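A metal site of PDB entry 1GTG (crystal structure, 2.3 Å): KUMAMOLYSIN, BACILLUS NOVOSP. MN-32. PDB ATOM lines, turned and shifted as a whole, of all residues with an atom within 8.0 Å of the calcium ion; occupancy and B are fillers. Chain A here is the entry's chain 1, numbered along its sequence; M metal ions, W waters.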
ATOM      1  N   VAL A 207       1.359 -35.077  -0.069  1.00  0.00           N
ATOM      2  CA  VAL A 207       0.085 -35.767  -0.075  1.00  0.00           C
ATOM      3  C   VAL A 207       0.270 -37.152   0.553  1.00  0.00           C
ATOM      4  O   VAL A 207       1.264 -37.827   0.300  1.00  0.00           O
ATOM      5  CB  VAL A 207      -0.453 -35.979  -1.524  1.00  0.00           C
ATOM      6  CG1 VAL A 207      -1.703 -36.837  -1.478  1.00  0.00           C
ATOM      7  CG2 VAL A 207      -0.749 -34.640  -2.197  1.00  0.00           C
ATOM      8  N   HIS A 315       0.029 -23.656   5.075  1.00  0.00           N
ATOM      9  CA  HIS A 315       1.242 -24.221   4.507  1.00  0.00           C
ATOM     10  C   HIS A 315       0.749 -24.961   3.272  1.00  0.00           C
ATOM     11  O   HIS A 315      -0.003 -25.913   3.389  1.00  0.00           O
ATOM     12  CB  HIS A 315       1.898 -25.225   5.442  1.00  0.00           C
ATOM     13  CG  HIS A 315       3.159 -25.790   4.891  1.00  0.00           C
ATOM     14  ND1 HIS A 315       3.452 -27.140   4.938  1.00  0.00           N
ATOM     15  CD2 HIS A 315       4.203 -25.201   4.273  1.00  0.00           C
ATOM     16  CE1 HIS A 315       4.627 -27.352   4.366  1.00  0.00           C
ATOM     17  NE2 HIS A 315       5.103 -26.198   3.958  1.00  0.00           N
ATOM     18  N   ASP A 316       1.145 -24.501   2.103  1.00  0.00           N
ATOM     19  CA  ASP A 316       0.735 -25.074   0.823  1.00  0.00           C
ATOM     20  C   ASP A 316       1.322 -26.473   0.551  1.00  0.00           C
ATOM     21  O   ASP A 316       2.525 -26.641   0.564  1.00  0.00           O
ATOM     22  CB  ASP A 316       1.183 -24.143  -0.309  1.00  0.00           C
ATOM     23  CG  ASP A 316       0.356 -24.297  -1.569  1.00  0.00           C
ATOM     24  OD1 ASP A 316      -0.218 -25.367  -1.761  1.00  0.00           O
ATOM     25  OD2 ASP A 316       0.290 -23.355  -2.379  1.00  0.00           O
ATOM     26  N   ILE A 317       0.486 -27.480   0.323  1.00  0.00           N
ATOM     27  CA  ILE A 317       1.041 -28.791  -0.014  1.00  0.00           C
ATOM     28  C   ILE A 317       0.985 -28.812  -1.542  1.00  0.00           C
ATOM     29  O   ILE A 317      -0.045 -28.624  -2.115  1.00  0.00           O
ATOM     30  CB  ILE A 317       0.217 -29.979   0.580  1.00  0.00           C
ATOM     31  CG1 ILE A 317       0.605 -30.234   2.036  1.00  0.00           C
ATOM     32  CG2 ILE A 317       0.558 -31.267  -0.129  1.00  0.00           C
ATOM     33  CD1 ILE A 317       0.505 -29.040   2.962  1.00  0.00           C
ATOM     34  N   THR A 318       2.110 -29.013  -2.196  1.00  0.00           N
ATOM     35  CA  THR A 318       2.145 -28.975  -3.657  1.00  0.00           C
ATOM     36  C   THR A 318       2.650 -30.241  -4.303  1.00  0.00           C
ATOM     37  O   THR A 318       2.662 -30.323  -5.519  1.00  0.00           O
ATOM     38  CB  THR A 318       3.085 -27.896  -4.134  1.00  0.00           C
ATOM     39  OG1 THR A 318       4.423 -28.255  -3.736  1.00  0.00           O
ATOM     40  CG2 THR A 318       2.707 -26.548  -3.513  1.00  0.00           C
ATOM     41  N   GLU A 319       3.094 -31.209  -3.499  1.00  0.00           N
ATOM     42  CA  GLU A 319       3.628 -32.462  -4.011  1.00  0.00           C
ATOM     43  C   GLU A 319       2.824 -33.706  -3.698  1.00  0.00           C
ATOM     44  O   GLU A 319       2.393 -33.917  -2.576  1.00  0.00           O
ATOM     45  CB  GLU A 319       5.048 -32.678  -3.473  1.00  0.00           C
ATOM     46  CG  GLU A 319       6.112 -31.814  -4.105  1.00  0.00           C
ATOM     47  CD  GLU A 319       7.508 -32.188  -3.597  1.00  0.00           C
ATOM     48  OE1 GLU A 319       7.793 -33.407  -3.532  1.00  0.00           O
ATOM     49  OE2 GLU A 319       8.317 -31.283  -3.274  1.00  0.00           O
ATOM     50  N   GLN A 332      -3.991 -34.532  -8.244  1.00  0.00           N
ATOM     51  CA  GLN A 332      -2.614 -34.328  -7.940  1.00  0.00           C
ATOM     52  C   GLN A 332      -2.652 -33.024  -7.157  1.00  0.00           C
ATOM     53  O   GLN A 332      -3.616 -32.262  -7.271  1.00  0.00           O
ATOM     54  CB  GLN A 332      -1.843 -34.136  -9.249  1.00  0.00           C
ATOM     55  CG  GLN A 332      -0.368 -34.465  -9.186  1.00  0.00           C
ATOM     56  CD  GLN A 332       0.310 -34.267 -10.533  1.00  0.00           C
ATOM     57  OE1 GLN A 332      -0.244 -34.646 -11.573  1.00  0.00           O
ATOM     58  NE2 GLN A 332       1.505 -33.691 -10.517  1.00  0.00           N
ATOM     59  N   ALA A 333      -1.625 -32.790  -6.347  1.00  0.00           N
ATOM     60  CA  ALA A 333      -1.523 -31.560  -5.581  1.00  0.00           C
ATOM     61  C   ALA A 333      -0.867 -30.538  -6.502  1.00  0.00           C
ATOM     62  O   ALA A 333      -0.243 -30.890  -7.500  1.00  0.00           O
ATOM     63  CB  ALA A 333      -0.663 -31.776  -4.337  1.00  0.00           C
ATOM     64  N   GLY A 334      -1.025 -29.267  -6.193  1.00  0.00           N
ATOM     65  CA  GLY A 334      -0.419 -28.256  -7.034  1.00  0.00           C
ATOM     66  C   GLY A 334      -0.364 -27.014  -6.210  1.00  0.00           C
ATOM     67  O   GLY A 334      -0.675 -27.066  -5.023  1.00  0.00           O
ATOM     68  N   PRO A 335       0.047 -25.891  -6.804  1.00  0.00           N
ATOM     69  CA  PRO A 335       0.098 -24.664  -5.998  1.00  0.00           C
ATOM     70  C   PRO A 335      -1.348 -24.219  -5.719  1.00  0.00           C
ATOM     71  O   PRO A 335      -2.206 -24.312  -6.599  1.00  0.00           O
ATOM     72  CB  PRO A 335       0.842 -23.703  -6.915  1.00  0.00           C
ATOM     73  CG  PRO A 335       0.415 -24.178  -8.316  1.00  0.00           C
ATOM     74  CD  PRO A 335       0.539 -25.673  -8.174  1.00  0.00           C
ATOM     75  N   GLY A 336      -1.626 -23.743  -4.507  1.00  0.00           N
ATOM     76  CA  GLY A 336      -2.973 -23.286  -4.195  1.00  0.00           C
ATOM     77  C   GLY A 336      -3.930 -24.422  -3.873  1.00  0.00           C
ATOM     78  O   GLY A 336      -3.515 -25.552  -3.742  1.00  0.00           O
ATOM     79  N   TRP A 337      -5.228 -24.135  -3.756  1.00  0.00           N
ATOM     80  CA  TRP A 337      -6.179 -25.212  -3.448  1.00  0.00           C
ATOM     81  C   TRP A 337      -6.014 -26.409  -4.418  1.00  0.00           C
ATOM     82  O   TRP A 337      -5.804 -26.209  -5.620  1.00  0.00           O
ATOM     83  CB  TRP A 337      -7.615 -24.666  -3.515  1.00  0.00           C
ATOM     84  CG  TRP A 337      -8.654 -25.633  -3.000  1.00  0.00           C
ATOM     85  CD1 TRP A 337      -9.188 -25.675  -1.739  1.00  0.00           C
ATOM     86  CD2 TRP A 337      -9.148 -26.797  -3.690  1.00  0.00           C
ATOM     87  NE1 TRP A 337      -9.974 -26.803  -1.590  1.00  0.00           N
ATOM     88  CE2 TRP A 337      -9.975 -27.509  -2.768  1.00  0.00           C
ATOM     89  CE3 TRP A 337      -8.974 -27.311  -4.983  1.00  0.00           C
ATOM     90  CZ2 TRP A 337     -10.613 -28.708  -3.112  1.00  0.00           C
ATOM     91  CZ3 TRP A 337      -9.615 -28.519  -5.324  1.00  0.00           C
ATOM     92  CH2 TRP A 337     -10.412 -29.201  -4.381  1.00  0.00           C
ATOM     93  N   ASP A 338      -6.051 -27.650  -3.907  1.00  0.00           N
ATOM     94  CA  ASP A 338      -5.977 -28.855  -4.756  1.00  0.00           C
ATOM     95  C   ASP A 338      -6.864 -29.964  -4.188  1.00  0.00           C
ATOM     96  O   ASP A 338      -7.158 -29.977  -3.000  1.00  0.00           O
ATOM     97  CB  ASP A 338      -4.541 -29.361  -4.964  1.00  0.00           C
ATOM     98  CG  ASP A 338      -3.866 -29.781  -3.685  1.00  0.00           C
ATOM     99  OD1 ASP A 338      -4.283 -30.783  -3.032  1.00  0.00           O
ATOM    100  OD2 ASP A 338      -2.892 -29.102  -3.346  1.00  0.00           O
ATOM    101  N   PRO A 339      -7.279 -30.939  -5.027  1.00  0.00           N
ATOM    102  CA  PRO A 339      -8.149 -32.031  -4.588  1.00  0.00           C
ATOM    103  C   PRO A 339      -7.523 -33.119  -3.765  1.00  0.00           C
ATOM    104  O   PRO A 339      -8.027 -34.229  -3.713  1.00  0.00           O
ATOM    105  CB  PRO A 339      -8.743 -32.562  -5.888  1.00  0.00           C
ATOM    106  CG  PRO A 339      -8.248 -31.578  -6.980  1.00  0.00           C
ATOM    107  CD  PRO A 339      -6.944 -31.105  -6.443  1.00  0.00           C
ATOM    108  N   CYS A 340      -6.413 -32.783  -3.099  1.00  0.00           N
ATOM    109  CA  CYS A 340      -5.725 -33.769  -2.276  1.00  0.00           C
ATOM    110  C   CYS A 340      -5.612 -33.218  -0.890  1.00  0.00           C
ATOM    111  O   CYS A 340      -5.810 -33.939   0.091  1.00  0.00           O
ATOM    112  CB  CYS A 340      -4.294 -34.025  -2.764  1.00  0.00           C
ATOM    113  SG  CYS A 340      -4.145 -34.832  -4.329  1.00  0.00           S
ATOM    114  N   THR A 341      -5.292 -31.928  -0.814  1.00  0.00           N
ATOM    115  CA  THR A 341      -5.073 -31.263   0.455  1.00  0.00           C
ATOM    116  C   THR A 341      -5.802 -29.943   0.616  1.00  0.00           C
ATOM    117  O   THR A 341      -5.637 -29.261   1.624  1.00  0.00           O
ATOM    118  CB  THR A 341      -3.573 -31.012   0.656  1.00  0.00           C
ATOM    119  OG1 THR A 341      -3.057 -30.247  -0.443  1.00  0.00           O
ATOM    120  CG2 THR A 341      -2.841 -32.344   0.724  1.00  0.00           C
ATOM    121  N   GLY A 342      -6.618 -29.580  -0.377  1.00  0.00           N
ATOM    122  CA  GLY A 342      -7.344 -28.333  -0.297  1.00  0.00           C
ATOM    123  C   GLY A 342      -6.420 -27.164  -0.029  1.00  0.00           C
ATOM    124  O   GLY A 342      -5.384 -27.037  -0.681  1.00  0.00           O
ATOM    125  N   LEU A 343      -6.776 -26.314   0.936  1.00  0.00           N
ATOM    126  CA  LEU A 343      -5.947 -25.150   1.263  1.00  0.00           C
ATOM    127  C   LEU A 343      -4.619 -25.523   1.967  1.00  0.00           C
ATOM    128  O   LEU A 343      -3.731 -24.671   2.147  1.00  0.00           O
ATOM    129  CB  LEU A 343      -6.754 -24.166   2.121  1.00  0.00           C
ATOM    130  CG  LEU A 343      -8.129 -23.727   1.568  1.00  0.00           C
ATOM    131  CD1 LEU A 343      -8.857 -22.883   2.613  1.00  0.00           C
ATOM    132  CD2 LEU A 343      -7.958 -22.929   0.262  1.00  0.00           C
ATOM    133  N   GLY A 344      -4.471 -26.797   2.332  1.00  0.00           N
ATOM    134  CA  GLY A 344      -3.259 -27.260   2.986  1.00  0.00           C
ATOM    135  C   GLY A 344      -3.384 -27.403   4.508  1.00  0.00           C
ATOM    136  O   GLY A 344      -4.483 -27.543   5.026  1.00  0.00           O
HETATM  137 CA    CA M   1      -1.795 -27.010  -2.795  1.00  0.00          CA
HETATM  138  O   HOH W   1      -2.835 -27.651  -0.589  1.00  0.00           O
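The calcium ion is bound by OD2 of Asp 338 (2.4 Å), O of Gly 336 (2.4 Å), O of Ile 317 (2.5 Å), O of Gly 334 (2.5 Å), OD1 of Asp 316 (2.5 Å) and water W1 (2.5 Å). The calcium ion has six donor atoms within binding distance.
Water W1 lies within hydrogen-bond range of OG1 of Thr 341 (2.6 Å), O of Gly 342 (2.6 Å), N of Ile 317 (3.4 Å) and N of Gly 344 (3.5 Å).
OD1 of Asp 338 is in hydrogen-bond range of N of Thr 341, at 2.7 Å. OD1 of Asp 338 is in hydrogen-bond range of N of Cys 340 (2.9 Å).
Five residues have an atom within 4 Å of the calcium ion: Asp 316, Ile 317, Gly 334, Gly 336 and Asp 338. The nearest printed residue that does not touch the calcium ion is Pro 335 (4.1 Å).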
